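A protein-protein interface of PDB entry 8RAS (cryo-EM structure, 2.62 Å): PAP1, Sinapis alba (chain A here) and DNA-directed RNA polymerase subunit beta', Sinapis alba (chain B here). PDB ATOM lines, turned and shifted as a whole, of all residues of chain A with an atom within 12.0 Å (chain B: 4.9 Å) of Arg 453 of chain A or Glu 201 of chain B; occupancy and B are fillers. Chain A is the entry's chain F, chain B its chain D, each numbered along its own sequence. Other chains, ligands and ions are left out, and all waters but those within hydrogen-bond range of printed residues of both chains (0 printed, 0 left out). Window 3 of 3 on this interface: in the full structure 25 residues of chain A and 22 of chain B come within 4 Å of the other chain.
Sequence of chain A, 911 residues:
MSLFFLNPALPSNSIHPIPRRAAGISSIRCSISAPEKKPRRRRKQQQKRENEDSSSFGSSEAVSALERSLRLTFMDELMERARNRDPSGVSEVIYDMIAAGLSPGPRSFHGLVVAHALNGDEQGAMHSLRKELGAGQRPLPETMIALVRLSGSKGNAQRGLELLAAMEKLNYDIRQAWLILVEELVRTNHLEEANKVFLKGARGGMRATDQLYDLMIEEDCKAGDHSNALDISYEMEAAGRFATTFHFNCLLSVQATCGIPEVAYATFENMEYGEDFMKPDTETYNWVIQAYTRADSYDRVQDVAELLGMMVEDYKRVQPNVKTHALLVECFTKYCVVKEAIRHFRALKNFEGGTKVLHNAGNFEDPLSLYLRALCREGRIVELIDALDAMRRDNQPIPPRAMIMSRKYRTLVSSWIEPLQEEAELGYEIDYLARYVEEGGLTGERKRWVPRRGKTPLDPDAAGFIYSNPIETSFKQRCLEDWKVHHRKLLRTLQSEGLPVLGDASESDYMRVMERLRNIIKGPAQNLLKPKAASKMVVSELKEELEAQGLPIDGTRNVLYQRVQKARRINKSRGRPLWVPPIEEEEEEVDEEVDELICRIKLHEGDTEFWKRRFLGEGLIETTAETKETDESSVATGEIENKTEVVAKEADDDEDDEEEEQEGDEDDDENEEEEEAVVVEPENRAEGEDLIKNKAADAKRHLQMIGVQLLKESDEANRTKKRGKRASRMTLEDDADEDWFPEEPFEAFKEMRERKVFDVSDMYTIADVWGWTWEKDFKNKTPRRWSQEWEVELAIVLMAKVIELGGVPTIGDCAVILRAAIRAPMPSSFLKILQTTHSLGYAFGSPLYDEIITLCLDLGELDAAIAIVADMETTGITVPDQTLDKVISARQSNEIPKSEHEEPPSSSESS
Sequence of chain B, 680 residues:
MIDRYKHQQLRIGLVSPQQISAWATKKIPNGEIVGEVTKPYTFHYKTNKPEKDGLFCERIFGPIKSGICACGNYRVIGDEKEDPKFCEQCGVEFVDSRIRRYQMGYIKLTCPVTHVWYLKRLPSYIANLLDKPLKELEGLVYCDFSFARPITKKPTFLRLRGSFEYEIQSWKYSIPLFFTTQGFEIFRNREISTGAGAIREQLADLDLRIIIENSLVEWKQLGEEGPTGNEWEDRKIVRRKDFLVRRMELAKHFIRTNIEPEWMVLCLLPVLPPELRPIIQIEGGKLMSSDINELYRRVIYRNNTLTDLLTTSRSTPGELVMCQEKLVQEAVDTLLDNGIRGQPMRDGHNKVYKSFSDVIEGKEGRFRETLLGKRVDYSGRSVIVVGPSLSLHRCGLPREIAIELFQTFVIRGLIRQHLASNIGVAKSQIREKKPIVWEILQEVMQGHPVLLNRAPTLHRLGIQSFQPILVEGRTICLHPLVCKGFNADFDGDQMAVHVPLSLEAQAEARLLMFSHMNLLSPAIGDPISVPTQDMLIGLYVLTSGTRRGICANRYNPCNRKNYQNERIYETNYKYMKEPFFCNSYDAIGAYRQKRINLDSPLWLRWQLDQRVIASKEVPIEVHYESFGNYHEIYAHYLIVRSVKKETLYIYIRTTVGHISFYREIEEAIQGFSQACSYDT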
ATOM      1  N   ARG A 448      32.564 -24.456 -36.146  1.00  0.00           N
ATOM      2  CA  ARG A 448      31.179 -24.156 -35.815  1.00  0.00           C
ATOM      3  C   ARG A 448      30.968 -22.647 -35.752  1.00  0.00           C
ATOM      4  O   ARG A 448      31.737 -21.929 -35.107  1.00  0.00           O
ATOM      5  CB  ARG A 448      30.806 -24.812 -34.486  1.00  0.00           C
ATOM      6  CG  ARG A 448      29.720 -25.863 -34.614  1.00  0.00           C
ATOM      7  CD  ARG A 448      30.247 -27.111 -35.306  1.00  0.00           C
ATOM      8  NE  ARG A 448      31.258 -27.806 -34.520  1.00  0.00           N
ATOM      9  CZ  ARG A 448      31.033 -28.904 -33.814  1.00  0.00           C
ATOM     10  NH1 ARG A 448      29.839 -29.474 -33.784  1.00  0.00           N
ATOM     11  NH2 ARG A 448      32.030 -29.449 -33.122  1.00  0.00           N
ATOM     12  N   TRP A 449      29.925 -22.170 -36.427  1.00  0.00           N
ATOM     13  CA  TRP A 449      29.657 -20.735 -36.545  1.00  0.00           C
ATOM     14  C   TRP A 449      28.652 -20.277 -35.487  1.00  0.00           C
ATOM     15  O   TRP A 449      27.579 -19.756 -35.790  1.00  0.00           O
ATOM     16  CB  TRP A 449      29.164 -20.407 -37.951  1.00  0.00           C
ATOM     17  CG  TRP A 449      30.248 -20.404 -38.980  1.00  0.00           C
ATOM     18  CD1 TRP A 449      30.932 -21.485 -39.452  1.00  0.00           C
ATOM     19  CD2 TRP A 449      30.772 -19.264 -39.668  1.00  0.00           C
ATOM     20  NE1 TRP A 449      31.852 -21.088 -40.392  1.00  0.00           N
ATOM     21  CE2 TRP A 449      31.774 -19.729 -40.542  1.00  0.00           C
ATOM     22  CE3 TRP A 449      30.494 -17.895 -39.629  1.00  0.00           C
ATOM     23  CZ2 TRP A 449      32.498 -18.874 -41.370  1.00  0.00           C
ATOM     24  CZ3 TRP A 449      31.213 -17.048 -40.452  1.00  0.00           C
ATOM     25  CH2 TRP A 449      32.203 -17.541 -41.311  1.00  0.00           C
ATOM     26  N   VAL A 450      29.019 -20.474 -34.231  1.00  0.00           N
ATOM     27  CA  VAL A 450      28.207 -20.070 -33.085  1.00  0.00           C
ATOM     28  C   VAL A 450      28.951 -18.970 -32.341  1.00  0.00           C
ATOM     29  O   VAL A 450      30.154 -19.114 -32.090  1.00  0.00           O
ATOM     30  CB  VAL A 450      27.908 -21.258 -32.150  1.00  0.00           C
ATOM     31  CG1 VAL A 450      29.156 -22.101 -31.942  1.00  0.00           C
ATOM     32  CG2 VAL A 450      27.360 -20.770 -30.818  1.00  0.00           C
ATOM     33  N   PRO A 451      28.296 -17.861 -31.992  1.00  0.00           N
ATOM     34  CA  PRO A 451      28.989 -16.805 -31.245  1.00  0.00           C
ATOM     35  C   PRO A 451      29.425 -17.292 -29.872  1.00  0.00           C
ATOM     36  O   PRO A 451      28.775 -18.134 -29.249  1.00  0.00           O
ATOM     37  CB  PRO A 451      27.937 -15.693 -31.137  1.00  0.00           C
ATOM     38  CG  PRO A 451      26.932 -15.999 -32.201  1.00  0.00           C
ATOM     39  CD  PRO A 451      26.913 -17.489 -32.325  1.00  0.00           C
ATOM     40  N   ARG A 452      30.544 -16.744 -29.400  1.00  0.00           N
ATOM     41  CA  ARG A 452      31.116 -17.133 -28.121  1.00  0.00           C
ATOM     42  C   ARG A 452      31.547 -15.892 -27.357  1.00  0.00           C
ATOM     43  O   ARG A 452      31.865 -14.857 -27.948  1.00  0.00           O
ATOM     44  CB  ARG A 452      32.311 -18.078 -28.301  1.00  0.00           C
ATOM     45  CG  ARG A 452      31.924 -19.521 -28.570  1.00  0.00           C
ATOM     46  CD  ARG A 452      30.848 -19.993 -27.606  1.00  0.00           C
ATOM     47  NE  ARG A 452      30.041 -21.067 -28.170  1.00  0.00           N
ATOM     48  CZ  ARG A 452      30.437 -22.328 -28.270  1.00  0.00           C
ATOM     49  NH1 ARG A 452      31.633 -22.713 -27.858  1.00  0.00           N
ATOM     50  NH2 ARG A 452      29.610 -23.227 -28.797  1.00  0.00           N
ATOM     51  N   ARG A 453      31.554 -16.007 -26.030  1.00  0.00           N
ATOM     52  CA  ARG A 453      31.954 -14.904 -25.167  1.00  0.00           C
ATOM     53  C   ARG A 453      33.470 -14.768 -25.187  1.00  0.00           C
ATOM     54  O   ARG A 453      34.191 -15.727 -24.889  1.00  0.00           O
ATOM     55  CB  ARG A 453      31.451 -15.132 -23.744  1.00  0.00           C
ATOM     56  CG  ARG A 453      29.979 -14.820 -23.549  1.00  0.00           C
ATOM     57  CD  ARG A 453      29.462 -15.404 -22.244  1.00  0.00           C
ATOM     58  NE  ARG A 453      28.608 -14.469 -21.520  1.00  0.00           N
ATOM     59  CZ  ARG A 453      27.365 -14.163 -21.866  1.00  0.00           C
ATOM     60  NH1 ARG A 453      26.785 -14.712 -22.921  1.00  0.00           N
ATOM     61  NH2 ARG A 453      26.683 -13.291 -21.129  1.00  0.00           N
ATOM     62  N   GLY A 454      33.951 -13.589 -25.534  1.00  0.00           N
ATOM     63  CA  GLY A 454      35.374 -13.325 -25.604  1.00  0.00           C
ATOM     64  C   GLY A 454      35.683 -12.340 -26.708  1.00  0.00           C
ATOM     65  O   GLY A 454      34.931 -12.164 -27.664  1.00  0.00           O
ATOM     66  N   LYS A 455      36.829 -11.678 -26.572  1.00  0.00           N
ATOM     67  CA  LYS A 455      37.277 -10.694 -27.554  1.00  0.00           C
ATOM     68  C   LYS A 455      38.102 -11.343 -28.662  1.00  0.00           C
ATOM     69  O   LYS A 455      39.229 -10.942 -28.951  1.00  0.00           O
ATOM     70  CB  LYS A 455      38.062  -9.587 -26.860  1.00  0.00           C
ATOM     71  CG  LYS A 455      39.127 -10.084 -25.899  1.00  0.00           C
ATOM     72  CD  LYS A 455      39.904  -8.926 -25.305  1.00  0.00           C
ATOM     73  CE  LYS A 455      39.074  -8.195 -24.267  1.00  0.00           C
ATOM     74  NZ  LYS A 455      39.884  -7.187 -23.535  1.00  0.00           N
ATOM     75  N   THR A 456      37.532 -12.361 -29.296  1.00  0.00           N
ATOM     76  CA  THR A 456      38.156 -13.028 -30.425  1.00  0.00           C
ATOM     77  C   THR A 456      37.172 -13.088 -31.583  1.00  0.00           C
ATOM     78  O   THR A 456      35.966 -13.242 -31.373  1.00  0.00           O
ATOM     79  CB  THR A 456      38.612 -14.448 -30.055  1.00  0.00           C
ATOM     80  OG1 THR A 456      39.084 -15.126 -31.227  1.00  0.00           O
ATOM     81  CG2 THR A 456      37.470 -15.241 -29.440  1.00  0.00           C
ATOM     82  N   PRO A 457      37.657 -12.954 -32.817  1.00  0.00           N
ATOM     83  CA  PRO A 457      36.743 -12.971 -33.966  1.00  0.00           C
ATOM     84  C   PRO A 457      36.232 -14.377 -34.242  1.00  0.00           C
ATOM     85  O   PRO A 457      37.002 -15.339 -34.285  1.00  0.00           O
ATOM     86  CB  PRO A 457      37.608 -12.449 -35.118  1.00  0.00           C
ATOM     87  CG  PRO A 457      39.006 -12.755 -34.708  1.00  0.00           C
ATOM     88  CD  PRO A 457      39.042 -12.643 -33.212  1.00  0.00           C
ATOM     89  N   LEU A 458      34.914 -14.491 -34.422  1.00  0.00           N
ATOM     90  CA  LEU A 458      34.344 -15.749 -34.887  1.00  0.00           C
ATOM     91  C   LEU A 458      34.742 -16.022 -36.332  1.00  0.00           C
ATOM     92  O   LEU A 458      34.997 -17.172 -36.706  1.00  0.00           O
ATOM     93  CB  LEU A 458      32.824 -15.722 -34.743  1.00  0.00           C
ATOM     94  CG  LEU A 458      32.064 -16.959 -35.224  1.00  0.00           C
ATOM     95  CD1 LEU A 458      32.466 -18.184 -34.420  1.00  0.00           C
ATOM     96  CD2 LEU A 458      30.565 -16.729 -35.142  1.00  0.00           C
ATOM     97  N   ASP A 459      34.805 -14.981 -37.147  1.00  0.00           N
ATOM     98  CA  ASP A 459      35.180 -15.120 -38.547  1.00  0.00           C
ATOM     99  C   ASP A 459      36.675 -15.391 -38.663  1.00  0.00           C
ATOM    100  O   ASP A 459      37.479 -14.583 -38.180  1.00  0.00           O
ATOM    101  CB  ASP A 459      34.805 -13.848 -39.305  1.00  0.00           C
ATOM    102  CG  ASP A 459      35.050 -13.955 -40.797  1.00  0.00           C
ATOM    103  OD1 ASP A 459      35.240 -15.081 -41.299  1.00  0.00           O
ATOM    104  OD2 ASP A 459      35.049 -12.904 -41.471  1.00  0.00           O
ATOM    105  N   PRO B 150      18.247  -9.719 -22.123  1.00  0.00           N
ATOM    106  CA  PRO B 150      19.569  -9.252 -21.686  1.00  0.00           C
ATOM    107  C   PRO B 150      20.724  -9.886 -22.438  1.00  0.00           C
ATOM    108  O   PRO B 150      21.802  -9.279 -22.500  1.00  0.00           O
ATOM    109  CB  PRO B 150      19.597  -9.645 -20.206  1.00  0.00           C
ATOM    110  CG  PRO B 150      18.785 -10.903 -20.163  1.00  0.00           C
ATOM    111  CD  PRO B 150      17.737 -10.799 -21.259  1.00  0.00           C
ATOM    112  N   ILE B 151      20.543 -11.077 -23.009  1.00  0.00           N
ATOM    113  CA  ILE B 151      21.617 -11.794 -23.680  1.00  0.00           C
ATOM    114  C   ILE B 151      21.167 -12.166 -25.086  1.00  0.00           C
ATOM    115  O   ILE B 151      19.973 -12.223 -25.390  1.00  0.00           O
ATOM    116  CB  ILE B 151      22.059 -13.049 -22.896  1.00  0.00           C
ATOM    117  CG1 ILE B 151      21.178 -14.245 -23.243  1.00  0.00           C
ATOM    118  CG2 ILE B 151      22.041 -12.791 -21.397  1.00  0.00           C
ATOM    119  CD1 ILE B 151      21.804 -15.563 -22.891  1.00  0.00           C
ATOM    120  N   LYS B 153      23.675 -14.347 -27.357  1.00  0.00           N
ATOM    121  CA  LYS B 153      24.363 -15.535 -27.854  1.00  0.00           C
ATOM    122  C   LYS B 153      23.642 -16.835 -27.523  1.00  0.00           C
ATOM    123  O   LYS B 153      24.184 -17.908 -27.815  1.00  0.00           O
ATOM    124  CB  LYS B 153      25.791 -15.581 -27.306  1.00  0.00           C
ATOM    125  CG  LYS B 153      26.698 -14.493 -27.857  1.00  0.00           C
ATOM    126  CD  LYS B 153      28.092 -14.583 -27.267  1.00  0.00           C
ATOM    127  CE  LYS B 153      28.928 -13.375 -27.654  1.00  0.00           C
ATOM    128  NZ  LYS B 153      28.796 -13.052 -29.101  1.00  0.00           N
ATOM    129  N   GLY B 197      23.120  -8.203 -12.293  1.00  0.00           N
ATOM    130  CA  GLY B 197      23.326  -9.429 -13.046  1.00  0.00           C
ATOM    131  C   GLY B 197      22.996  -9.266 -14.517  1.00  0.00           C
ATOM    132  O   GLY B 197      23.717  -9.762 -15.385  1.00  0.00           O
ATOM    133  N   ALA B 198      21.904  -8.559 -14.817  1.00  0.00           N
ATOM    134  CA  ALA B 198      21.564  -8.273 -16.206  1.00  0.00           C
ATOM    135  C   ALA B 198      22.639  -7.426 -16.869  1.00  0.00           C
ATOM    136  O   ALA B 198      22.984  -7.648 -18.036  1.00  0.00           O
ATOM    137  CB  ALA B 198      20.207  -7.574 -16.283  1.00  0.00           C
ATOM    138  N   ILE B 199      23.179  -6.447 -16.141  1.00  0.00           N
ATOM    139  CA  ILE B 199      24.244  -5.611 -16.687  1.00  0.00           C
ATOM    140  C   ILE B 199      25.467  -6.454 -17.009  1.00  0.00           C
ATOM    141  O   ILE B 199      26.076  -6.315 -18.078  1.00  0.00           O
ATOM    142  CB  ILE B 199      24.590  -4.481 -15.702  1.00  0.00           C
ATOM    143  CG1 ILE B 199      23.616  -3.318 -15.843  1.00  0.00           C
ATOM    144  CG2 ILE B 199      25.996  -3.974 -15.949  1.00  0.00           C
ATOM    145  CD1 ILE B 199      23.957  -2.167 -14.932  1.00  0.00           C
ATOM    146  N   ARG B 200      25.850  -7.341 -16.090  1.00  0.00           N
ATOM    147  CA  ARG B 200      27.019  -8.184 -16.314  1.00  0.00           C
ATOM    148  C   ARG B 200      26.796  -9.130 -17.487  1.00  0.00           C
ATOM    149  O   ARG B 200      27.720  -9.390 -18.267  1.00  0.00           O
ATOM    150  CB  ARG B 200      27.356  -8.965 -15.045  1.00  0.00           C
ATOM    151  CG  ARG B 200      28.682  -9.694 -15.112  1.00  0.00           C
ATOM    152  CD  ARG B 200      29.240  -9.952 -13.727  1.00  0.00           C
ATOM    153  NE  ARG B 200      30.696 -10.006 -13.725  1.00  0.00           N
ATOM    154  CZ  ARG B 200      31.409 -11.045 -14.140  1.00  0.00           C
ATOM    155  NH1 ARG B 200      30.830 -12.140 -14.604  1.00  0.00           N
ATOM    156  NH2 ARG B 200      32.736 -10.984 -14.086  1.00  0.00           N
ATOM    157  N   GLU B 201      25.579  -9.660 -17.624  1.00  0.00           N
ATOM    158  CA  GLU B 201      25.273 -10.515 -18.767  1.00  0.00           C
ATOM    159  C   GLU B 201      25.350  -9.738 -20.076  1.00  0.00           C
ATOM    160  O   GLU B 201      25.847 -10.255 -21.083  1.00  0.00           O
ATOM    161  CB  GLU B 201      23.892 -11.144 -18.596  1.00  0.00           C
ATOM    162  CG  GLU B 201      23.815 -12.179 -17.486  1.00  0.00           C
ATOM    163  CD  GLU B 201      24.888 -13.240 -17.603  1.00  0.00           C
ATOM    164  OE1 GLU B 201      24.972 -13.892 -18.665  1.00  0.00           O
ATOM    165  OE2 GLU B 201      25.650 -13.424 -16.629  1.00  0.00           O
ATOM    166  N   GLN B 202      24.856  -8.497 -20.083  1.00  0.00           N
ATOM    167  CA  GLN B 202      24.939  -7.676 -21.287  1.00  0.00           C
ATOM    168  C   GLN B 202      26.386  -7.356 -21.641  1.00  0.00           C
ATOM    169  O   GLN B 202      26.753  -7.324 -22.821  1.00  0.00           O
ATOM    170  CB  GLN B 202      24.141  -6.385 -21.104  1.00  0.00           C
ATOM    171  CG  GLN B 202      22.641  -6.585 -21.007  1.00  0.00           C
ATOM    172  CD  GLN B 202      21.912  -5.323 -20.595  1.00  0.00           C
ATOM    173  OE1 GLN B 202      21.933  -4.320 -21.309  1.00  0.00           O
ATOM    174  NE2 GLN B 202      21.262  -5.365 -19.440  1.00  0.00           N
ATOM    175  N   LEU B 203      27.218  -7.093 -20.633  1.00  0.00           N
ATOM    176  CA  LEU B 203      28.615  -6.768 -20.899  1.00  0.00           C
ATOM    177  C   LEU B 203      29.409  -7.989 -21.342  1.00  0.00           C
ATOM    178  O   LEU B 203      30.324  -7.865 -22.165  1.00  0.00           O
ATOM    179  CB  LEU B 203      29.260  -6.140 -19.663  1.00  0.00           C
ATOM    180  CG  LEU B 203      28.663  -4.836 -19.132  1.00  0.00           C
ATOM    181  CD1 LEU B 203      29.261  -4.489 -17.780  1.00  0.00           C
ATOM    182  CD2 LEU B 203      28.864  -3.697 -20.114  1.00  0.00           C
ATOM    183  N   ALA B 204      29.081  -9.170 -20.812  1.00  0.00           N
ATOM    184  CA  ALA B 204      29.871 -10.361 -21.106  1.00  0.00           C
ATOM    185  C   ALA B 204      29.743 -10.783 -22.566  1.00  0.00           C
ATOM    186  O   ALA B 204      30.731 -11.192 -23.185  1.00  0.00           O
ATOM    187  CB  ALA B 204      29.457 -11.503 -20.180  1.00  0.00           C
ATOM    188  N   ASP B 205      28.542 -10.697 -23.133  1.00  0.00           N
ATOM    189  CA  ASP B 205      28.296 -11.164 -24.491  1.00  0.00           C
ATOM    190  C   ASP B 205      28.419 -10.060 -25.535  1.00  0.00           C
ATOM    191  O   ASP B 205      28.085 -10.290 -26.702  1.00  0.00           O
ATOM    192  CB  ASP B 205      26.915 -11.819 -24.587  1.00  0.00           C
ATOM    193  CG  ASP B 205      25.785 -10.856 -24.287  1.00  0.00           C
ATOM    194  OD1 ASP B 205      26.057  -9.704 -23.897  1.00  0.00           O
ATOM    195  OD2 ASP B 205      24.615 -11.252 -24.451  1.00  0.00           O
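The guanidinium group of Arg 453 of chain A is in salt-bridge range of the side-chain carboxylate of Glu 201 of chain B, at 3.1 Å.
The backbone carbonyl oxygen (O) of Gln 202 of chain B sits close to the side-chain carboxylate (OD1) of Asp 205 of chain B (2.7 Å).
Lys 153 of chain B touches Pro 451 of chain A. Arg 452 of chain A touches Lys 153 of chain B (O to CE, 3.3 Å). Arg 453 of chain A touches Lys 153 of chain B (N to CD, 3.9 Å). Ala 204 of chain B touches Arg 453 of chain A. Arg 453 of chain A touches Asp 205 of chain B.
Of the printed residues of chain B, Pro 451 of chain A touches Lys 153 (3.4 Å). Of the printed residues of chain B, Arg 452 of chain A touches Lys 153 (3.3 Å). Of chain B, only Lys 153 (3.9 Å), Glu 201 (3.1 Å), Ala 204 (3.4 Å) and Asp 205 (3.3 Å) come within 4 Å of Arg 453 of chain A. No residue of chain A comes within 4 Å of Pro 150 of chain B. Of chain A, only Pro 451, Arg 452 and Arg 453 come within 4 Å of Lys 153 of chain B. No residue of chain A comes within 4 Å of Ala 198 of chain B. No residue of chain A comes within 4 Å of Arg 200 of chain B. No residue of chain A comes within 4 Å of Gln 202 of chain B. No residue of chain A comes within 4 Å of Leu 203 of chain B. Ala 204 of chain B touches just one residue of chain A: Arg 453 (3.4 Å). Of chain A, only Arg 453 (3.3 Å) comes within 4 Å of Asp 205 of chain B. The nearest residue of chain B that does not touch Arg 453 of chain A is Ile 151 of chain B (4.7 Å).
Printed residues of chain B that touch a printed residue of chain A: Lys 153, Glu 201, Ala 204 and Asp 205. Hydrophobic or aromatic side chains of chain B that line the printed part of chain A: Ala 204. Of the 12 printed residues of chain A, 3 touch a printed residue of chain B. Printed residues of chain A that touch a printed residue of chain B: Pro 451, Arg 452 and Arg 453. Among the printed residues, 6 pairs touch across the chains. Among the printed residues, Asp or Glu carboxylates within 4 Å of a Lys or Arg side-chain nitrogen of the other chain: Arg 453 of chain A with Glu 201 of chain B (3.1 Å).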
